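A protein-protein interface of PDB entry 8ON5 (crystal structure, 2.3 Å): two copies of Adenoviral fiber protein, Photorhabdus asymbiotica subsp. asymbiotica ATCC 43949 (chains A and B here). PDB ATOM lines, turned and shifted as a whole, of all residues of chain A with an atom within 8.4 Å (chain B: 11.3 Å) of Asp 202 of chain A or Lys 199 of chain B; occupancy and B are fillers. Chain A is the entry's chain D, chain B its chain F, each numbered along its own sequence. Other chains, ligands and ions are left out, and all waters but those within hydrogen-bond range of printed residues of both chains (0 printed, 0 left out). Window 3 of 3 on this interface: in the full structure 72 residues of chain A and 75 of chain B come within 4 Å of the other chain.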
ATOM      1  N   ASP A 197       1.592  -6.171   7.739  1.00  0.00           N
ATOM      2  CA  ASP A 197       2.471  -7.224   8.233  1.00  0.00           C
ATOM      3  C   ASP A 197       2.273  -7.316   9.743  1.00  0.00           C
ATOM      4  O   ASP A 197       2.726  -6.448  10.482  1.00  0.00           O
ATOM      5  CB  ASP A 197       3.926  -6.924   7.827  1.00  0.00           C
ATOM      6  CG  ASP A 197       5.033  -7.852   8.338  1.00  0.00           C
ATOM      7  OD1 ASP A 197       4.735  -8.932   8.888  1.00  0.00           O
ATOM      8  OD2 ASP A 197       6.215  -7.467   8.184  1.00  0.00           O
ATOM      9  N   ASN A 198       1.594  -8.366  10.206  1.00  0.00           N
ATOM     10  CA  ASN A 198       1.313  -8.486  11.630  1.00  0.00           C
ATOM     11  C   ASN A 198       2.499  -9.060  12.421  1.00  0.00           C
ATOM     12  O   ASN A 198       2.543  -8.875  13.637  1.00  0.00           O
ATOM     13  CB  ASN A 198       0.012  -9.257  11.851  1.00  0.00           C
ATOM     14  CG  ASN A 198      -1.170  -8.491  11.303  1.00  0.00           C
ATOM     15  OD1 ASN A 198      -1.275  -7.287  11.535  1.00  0.00           O
ATOM     16  ND2 ASN A 198      -2.031  -9.166  10.555  1.00  0.00           N
ATOM     17  N   LYS A 199       3.448  -9.734  11.744  1.00  0.00           N
ATOM     18  CA  LYS A 199       4.670 -10.240  12.364  1.00  0.00           C
ATOM     19  C   LYS A 199       5.563  -9.079  12.815  1.00  0.00           C
ATOM     20  O   LYS A 199       5.800  -8.897  14.005  1.00  0.00           O
ATOM     21  N   ASN A 200       6.055  -8.284  11.861  1.00  0.00           N
ATOM     22  CA  ASN A 200       7.037  -7.251  12.152  1.00  0.00           C
ATOM     23  C   ASN A 200       6.485  -5.875  11.788  1.00  0.00           C
ATOM     24  O   ASN A 200       7.215  -5.062  11.231  1.00  0.00           O
ATOM     25  N   GLY A 201       5.200  -5.634  12.099  1.00  0.00           N
ATOM     26  CA  GLY A 201       4.577  -4.322  11.956  1.00  0.00           C
ATOM     27  C   GLY A 201       4.814  -3.458  13.195  1.00  0.00           C
ATOM     28  O   GLY A 201       5.251  -3.967  14.221  1.00  0.00           O
ATOM     29  N   ASP A 202       4.527  -2.154  13.092  1.00  0.00           N
ATOM     30  CA  ASP A 202       4.905  -1.196  14.124  1.00  0.00           C
ATOM     31  C   ASP A 202       3.740  -0.304  14.593  1.00  0.00           C
ATOM     32  O   ASP A 202       3.836   0.232  15.704  1.00  0.00           O
ATOM     33  CB  ASP A 202       6.092  -0.362  13.633  1.00  0.00           C
ATOM     34  CG  ASP A 202       5.743   0.719  12.620  1.00  0.00           C
ATOM     35  OD1 ASP A 202       5.011   1.652  12.990  1.00  0.00           O
ATOM     36  OD2 ASP A 202       6.226   0.643  11.476  1.00  0.00           O
ATOM     37  N   THR A 203       2.672  -0.128  13.771  1.00  0.00           N
ATOM     38  CA  THR A 203       1.553   0.760  14.075  1.00  0.00           C
ATOM     39  C   THR A 203       0.215   0.037  13.883  1.00  0.00           C
ATOM     40  O   THR A 203      -0.083  -0.449  12.777  1.00  0.00           O
ATOM     41  CB  THR A 203       1.591   2.016  13.193  1.00  0.00           C
ATOM     42  OG1 THR A 203       2.804   2.714  13.466  1.00  0.00           O
ATOM     43  CG2 THR A 203       0.413   2.942  13.413  1.00  0.00           C
ATOM     44  N   GLU A 204      -0.606   0.017  14.956  1.00  0.00           N
ATOM     45  CA  GLU A 204      -1.841  -0.756  15.025  1.00  0.00           C
ATOM     46  C   GLU A 204      -3.013   0.013  14.397  1.00  0.00           C
ATOM     47  O   GLU A 204      -3.277   1.166  14.738  1.00  0.00           O
ATOM     48  CB  GLU A 204      -2.143  -1.118  16.489  1.00  0.00           C
ATOM     49  CG  GLU A 204      -3.289  -2.107  16.680  1.00  0.00           C
ATOM     50  CD  GLU A 204      -3.551  -2.611  18.098  1.00  0.00           C
ATOM     51  OE1 GLU A 204      -3.953  -1.812  18.988  1.00  0.00           O
ATOM     52  OE2 GLU A 204      -3.407  -3.827  18.302  1.00  0.00           O
ATOM     53  N   ILE A 205      -3.728  -0.647  13.479  1.00  0.00           N
ATOM     54  CA  ILE A 205      -4.942  -0.106  12.897  1.00  0.00           C
ATOM     55  C   ILE A 205      -6.131  -0.902  13.446  1.00  0.00           C
ATOM     56  O   ILE A 205      -6.191  -2.112  13.288  1.00  0.00           O
ATOM     57  CB  ILE A 205      -4.880  -0.169  11.356  1.00  0.00           C
ATOM     58  CG1 ILE A 205      -3.552   0.324  10.767  1.00  0.00           C
ATOM     59  CG2 ILE A 205      -6.065   0.568  10.764  1.00  0.00           C
ATOM     60  CD1 ILE A 205      -3.198   1.748  11.122  1.00  0.00           C
ATOM     61  N   LYS B 180      -5.786   4.748  17.659  1.00  0.00           N
ATOM     62  CA  LYS B 180      -5.419   5.982  16.982  1.00  0.00           C
ATOM     63  C   LYS B 180      -6.091   6.050  15.610  1.00  0.00           C
ATOM     64  O   LYS B 180      -6.423   7.130  15.126  1.00  0.00           O
ATOM     65  CB  LYS B 180      -3.893   5.989  16.852  1.00  0.00           C
ATOM     66  CG  LYS B 180      -3.275   7.052  15.955  1.00  0.00           C
ATOM     67  CD  LYS B 180      -3.256   8.437  16.562  1.00  0.00           C
ATOM     68  CE  LYS B 180      -1.988   9.193  16.218  1.00  0.00           C
ATOM     69  NZ  LYS B 180      -1.627   9.059  14.784  1.00  0.00           N
ATOM     70  N   TYR B 181      -6.222   4.873  14.980  1.00  0.00           N
ATOM     71  CA  TYR B 181      -6.781   4.695  13.654  1.00  0.00           C
ATOM     72  C   TYR B 181      -7.943   3.710  13.720  1.00  0.00           C
ATOM     73  O   TYR B 181      -7.757   2.567  14.160  1.00  0.00           O
ATOM     74  CB  TYR B 181      -5.723   4.139  12.706  1.00  0.00           C
ATOM     75  CG  TYR B 181      -4.595   5.082  12.372  1.00  0.00           C
ATOM     76  CD1 TYR B 181      -4.824   6.217  11.612  1.00  0.00           C
ATOM     77  CD2 TYR B 181      -3.295   4.839  12.799  1.00  0.00           C
ATOM     78  CE1 TYR B 181      -3.795   7.077  11.263  1.00  0.00           C
ATOM     79  CE2 TYR B 181      -2.256   5.699  12.464  1.00  0.00           C
ATOM     80  CZ  TYR B 181      -2.504   6.820  11.689  1.00  0.00           C
ATOM     81  OH  TYR B 181      -1.505   7.700  11.336  1.00  0.00           O
ATOM     82  N   THR B 193      -7.733  -6.071  14.319  1.00  0.00           N
ATOM     83  CA  THR B 193      -6.638  -5.129  14.138  1.00  0.00           C
ATOM     84  C   THR B 193      -5.673  -5.721  13.122  1.00  0.00           C
ATOM     85  O   THR B 193      -5.599  -6.949  12.982  1.00  0.00           O
ATOM     86  CB  THR B 193      -5.900  -4.808  15.444  1.00  0.00           C
ATOM     87  OG1 THR B 193      -5.116  -5.937  15.804  1.00  0.00           O
ATOM     88  CG2 THR B 193      -6.811  -4.473  16.601  1.00  0.00           C
ATOM     89  N   PHE B 194      -5.024  -4.828  12.360  1.00  0.00           N
ATOM     90  CA  PHE B 194      -3.857  -5.193  11.580  1.00  0.00           C
ATOM     91  C   PHE B 194      -2.791  -4.169  11.940  1.00  0.00           C
ATOM     92  O   PHE B 194      -3.093  -3.201  12.642  1.00  0.00           O
ATOM     93  CB  PHE B 194      -4.182  -5.376  10.090  1.00  0.00           C
ATOM     94  CG  PHE B 194      -4.624  -4.142   9.337  1.00  0.00           C
ATOM     95  CD1 PHE B 194      -3.706  -3.199   8.904  1.00  0.00           C
ATOM     96  CD2 PHE B 194      -5.962  -3.918   9.060  1.00  0.00           C
ATOM     97  CE1 PHE B 194      -4.115  -2.071   8.213  1.00  0.00           C
ATOM     98  CE2 PHE B 194      -6.367  -2.779   8.382  1.00  0.00           C
ATOM     99  CZ  PHE B 194      -5.442  -1.858   7.957  1.00  0.00           C
ATOM    100  N   TRP B 195      -1.551  -4.454  11.522  1.00  0.00           N
ATOM    101  CA  TRP B 195      -0.413  -3.609  11.826  1.00  0.00           C
ATOM    102  C   TRP B 195       0.216  -3.126  10.529  1.00  0.00           C
ATOM    103  O   TRP B 195       0.564  -3.931   9.667  1.00  0.00           O
ATOM    104  CB  TRP B 195       0.599  -4.378  12.677  1.00  0.00           C
ATOM    105  CG  TRP B 195       0.146  -4.664  14.076  1.00  0.00           C
ATOM    106  CD1 TRP B 195      -0.616  -5.715  14.494  1.00  0.00           C
ATOM    107  CD2 TRP B 195       0.491  -3.919  15.260  1.00  0.00           C
ATOM    108  NE1 TRP B 195      -0.791  -5.653  15.851  1.00  0.00           N
ATOM    109  CE2 TRP B 195      -0.115  -4.570  16.347  1.00  0.00           C
ATOM    110  CE3 TRP B 195       1.254  -2.776  15.508  1.00  0.00           C
ATOM    111  CZ2 TRP B 195       0.006  -4.098  17.655  1.00  0.00           C
ATOM    112  CZ3 TRP B 195       1.366  -2.303  16.795  1.00  0.00           C
ATOM    113  CH2 TRP B 195       0.752  -2.960  17.854  1.00  0.00           C
ATOM    114  N   ALA B 196       0.351  -1.806  10.403  1.00  0.00           N
ATOM    115  CA  ALA B 196       1.058  -1.225   9.279  1.00  0.00           C
ATOM    116  C   ALA B 196       2.537  -1.071   9.628  1.00  0.00           C
ATOM    117  O   ALA B 196       2.865  -0.796  10.785  1.00  0.00           O
ATOM    118  CB  ALA B 196       0.454   0.105   8.948  1.00  0.00           C
ATOM    119  N   ASP B 197       3.400  -1.215   8.607  1.00  0.00           N
ATOM    120  CA  ASP B 197       4.850  -1.122   8.755  1.00  0.00           C
ATOM    121  C   ASP B 197       5.324   0.282   8.371  1.00  0.00           C
ATOM    122  O   ASP B 197       5.791   0.479   7.249  1.00  0.00           O
ATOM    123  CB  ASP B 197       5.527  -2.217   7.914  1.00  0.00           C
ATOM    124  CG  ASP B 197       7.036  -2.356   8.073  1.00  0.00           C
ATOM    125  OD1 ASP B 197       7.655  -1.454   8.669  1.00  0.00           O
ATOM    126  OD2 ASP B 197       7.582  -3.385   7.596  1.00  0.00           O
ATOM    127  N   ASN B 198       5.210   1.242   9.307  1.00  0.00           N
ATOM    128  CA  ASN B 198       5.712   2.592   9.096  1.00  0.00           C
ATOM    129  C   ASN B 198       7.218   2.563   8.858  1.00  0.00           C
ATOM    130  O   ASN B 198       7.692   3.212   7.923  1.00  0.00           O
ATOM    131  CB  ASN B 198       5.398   3.551  10.251  1.00  0.00           C
ATOM    132  CG  ASN B 198       4.215   4.458   9.983  1.00  0.00           C
ATOM    133  OD1 ASN B 198       3.763   4.599   8.848  1.00  0.00           O
ATOM    134  ND2 ASN B 198       3.723   5.105  11.027  1.00  0.00           N
ATOM    135  N   LYS B 199       7.940   1.828   9.725  1.00  0.00           N
ATOM    136  CA  LYS B 199       9.373   1.587   9.598  1.00  0.00           C
ATOM    137  C   LYS B 199       9.766   1.564   8.127  1.00  0.00           C
ATOM    138  O   LYS B 199      10.312   2.537   7.624  1.00  0.00           O
ATOM    139  N   ASN B 200       9.426   0.478   7.424  1.00  0.00           N
ATOM    140  CA  ASN B 200      10.073   0.163   6.156  1.00  0.00           C
ATOM    141  C   ASN B 200       9.059  -0.054   5.034  1.00  0.00           C
ATOM    142  O   ASN B 200       9.402  -0.611   3.996  1.00  0.00           O
ATOM    143  CB  ASN B 200      10.992  -1.057   6.315  1.00  0.00           C
ATOM    144  CG  ASN B 200      11.846  -0.964   7.566  1.00  0.00           C
ATOM    145  OD1 ASN B 200      12.449   0.076   7.838  1.00  0.00           O
ATOM    146  ND2 ASN B 200      11.858  -2.017   8.366  1.00  0.00           N
ATOM    147  N   GLY B 201       7.811   0.390   5.236  1.00  0.00           N
ATOM    148  CA  GLY B 201       6.785   0.290   4.213  1.00  0.00           C
ATOM    149  C   GLY B 201       6.958   1.370   3.147  1.00  0.00           C
ATOM    150  O   GLY B 201       7.385   2.488   3.437  1.00  0.00           O
ATOM    151  N   ASP B 202       6.539   1.039   1.926  1.00  0.00           N
ATOM    152  CA  ASP B 202       6.902   1.792   0.740  1.00  0.00           C
ATOM    153  C   ASP B 202       5.703   2.503   0.115  1.00  0.00           C
ATOM    154  O   ASP B 202       5.782   2.888  -1.047  1.00  0.00           O
ATOM    155  CB  ASP B 202       7.462   0.830  -0.308  1.00  0.00           C
ATOM    156  CG  ASP B 202       6.495  -0.308  -0.585  1.00  0.00           C
ATOM    157  OD1 ASP B 202       6.449  -1.278   0.241  1.00  0.00           O
ATOM    158  OD2 ASP B 202       5.748  -0.177  -1.569  1.00  0.00           O
ATOM    159  N   THR B 203       4.592   2.645   0.853  1.00  0.00           N
ATOM    160  CA  THR B 203       3.328   3.107   0.283  1.00  0.00           C
ATOM    161  C   THR B 203       2.563   3.906   1.333  1.00  0.00           C
ATOM    162  O   THR B 203       2.156   3.333   2.343  1.00  0.00           O
ATOM    163  CB  THR B 203       2.469   1.923  -0.200  1.00  0.00           C
ATOM    164  OG1 THR B 203       3.178   1.185  -1.205  1.00  0.00           O
ATOM    165  CG2 THR B 203       1.124   2.357  -0.749  1.00  0.00           C
ATOM    166  N   GLU B 204       2.384   5.216   1.097  1.00  0.00           N
ATOM    167  CA  GLU B 204       1.799   6.101   2.101  1.00  0.00           C
ATOM    168  C   GLU B 204       0.275   6.025   2.002  1.00  0.00           C
ATOM    169  O   GLU B 204      -0.279   5.931   0.913  1.00  0.00           O
ATOM    170  CB  GLU B 204       2.312   7.538   1.961  1.00  0.00           C
ATOM    171  CG  GLU B 204       2.286   8.312   3.273  1.00  0.00           C
ATOM    172  CD  GLU B 204       2.838   9.743   3.256  1.00  0.00           C
ATOM    173  OE1 GLU B 204       3.243  10.223   2.175  1.00  0.00           O
ATOM    174  OE2 GLU B 204       2.856  10.401   4.335  1.00  0.00           O
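The side-chain carboxylate (OD1) of Asp 197 of chain A sits at hydrogen-bond distance from the backbone NH (N) of Lys 199 of chain A, 3.2 Å away.
OD1 of Asp 197 of chain A lies within hydrogen-bond range of N of Asn 200 of chain A, at 3.3 Å.
The side-chain hydroxyl of Thr 203 of chain A is in hydrogen-bond range of the side-chain carboxylate of Asp 202 of chain A (2.5 Å).
OD1 of Asp 197 of chain B sits close to N of Lys 199 of chain B (3.5 Å).
The backbone NH of Asn 200 of chain B sits at hydrogen-bond distance from the side-chain carboxylate of Asp 197 of chain B, 2.9 Å away.
Printed residues of chain B that touch a printed residue of chain A: Tyr 181, Thr 193, Phe 194, Trp 195, Ala 196, Asp 197, Asn 198 and Lys 199.
Hydrophobic or aromatic side chains of chain B within 4 Å of the printed part of chain A: Tyr 181, Phe 194, Trp 195 and Ala 196.
Among the printed residues, 18 pairs touch across the chains.
Among the printed residues, no Asp or Glu carboxylate lies within 4 Å of a Lys or Arg side-chain nitrogen of the other chain.
Phe 194 of chain B touches Asn 198 of chain A (CA to OD1, 3.3 Å).
Trp 195 of chain B touches Asp 202 of chain A.
CE2 of Tyr 181 of chain B touches CG2 of Thr 203 of chain A, 3.95 Å away.
Thr 203 of chain A touches Trp 195 of chain B.
OG1 of Thr 203 of chain A touches ND2 of Asn 198 of chain B, at 3.5 Å.
Glu 204 of chain A touches Thr 193 of chain B.
Phe 194 of chain B touches Glu 204 of chain A.
Glu 204 of chain A touches Trp 195 of chain B.
CD1 of Ile 205 of chain A touches CD2 of Tyr 181 of chain B, 3.5 Å away.
Thr 193 of chain B touches Ile 205 of chain A (CA to O, 3.2 Å).
Asp 202 of chain A touches Asp 197 of chain B, but with the chains exchanged Asp 197 of chain A does not touch Asp 202 of chain B (9.8 Å).
Asp 202 of chain A touches Asn 198 of chain B, but with the chains exchanged Asn 198 of chain A does not touch Asp 202 of chain B (13.2 Å).
Asp 202 of chain A touches Lys 199 of chain B, but with the chains exchanged Lys 199 of chain A does not touch Asp 202 of chain B (14.6 Å).
Thr 203 of chain A touches Asn 198 of chain B, but with the chains exchanged Asn 198 of chain A does not touch Thr 203 of chain B (14.1 Å).
Printed residues of chain B within 4 Å of Asp 202 of chain A: Trp 195 (3.6 Å), Ala 196 (3.2 Å), Asp 197 (3.3 Å), Asn 198 (2.5 Å) and Lys 199 (2.7 Å).
Of the printed residues of chain A, Lys 199 of chain B touches Asp 202 (2.7 Å).
No residue of chain B comes within 4 Å of Gly 201 of chain A.
Printed residues of chain A within 4 Å of Phe 194 of chain B: Asn 198, Glu 204 and Ile 205.
Printed residues of chain A within 4 Å of Tyr 181 of chain B: Thr 203 and Ile 205.
Printed residues of chain B within 4 Å of Ile 205 of chain A: Tyr 181, Thr 193 and Phe 194.
Printed residues of chain B within 4 Å of Glu 204 of chain A: Thr 193, Phe 194 and Trp 195.
Glu 204 of chain B touches none of the printed residues of chain A.
The nearest printed residue of chain A that does not touch Phe 194 of chain B is Thr 203 of chain A (4.1 Å).
N of Asp 197 of chain A sits at hydrogen-bond distance from O of Trp 195 of chain B (3.1 Å).
The backbone NH of Trp 195 of chain B lies within hydrogen-bond range of the side-chain amide oxygen of Asn 198 of chain A (2.8 Å).
O of Ala 196 of chain B is in hydrogen-bond range of N of Asp 202 of chain A, at 3.2 Å.
The side-chain carboxylate (OD2) of Asp 202 of chain A is in hydrogen-bond range of the backbone NH (N) of Asn 198 of chain B, at 2.5 Å.
The side-chain carboxylate (OD2) of Asp 202 of chain A lies within hydrogen-bond range of the backbone NH (N) of Lys 199 of chain B (2.7 Å).
The backbone carbonyl oxygen (O) of Thr 203 of chain A lies within hydrogen-bond range of the backbone NH (N) of Ala 196 of chain B (2.8 Å).
N of Ile 205 of chain A sits at hydrogen-bond distance from O of Phe 194 of chain B (2.8 Å).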
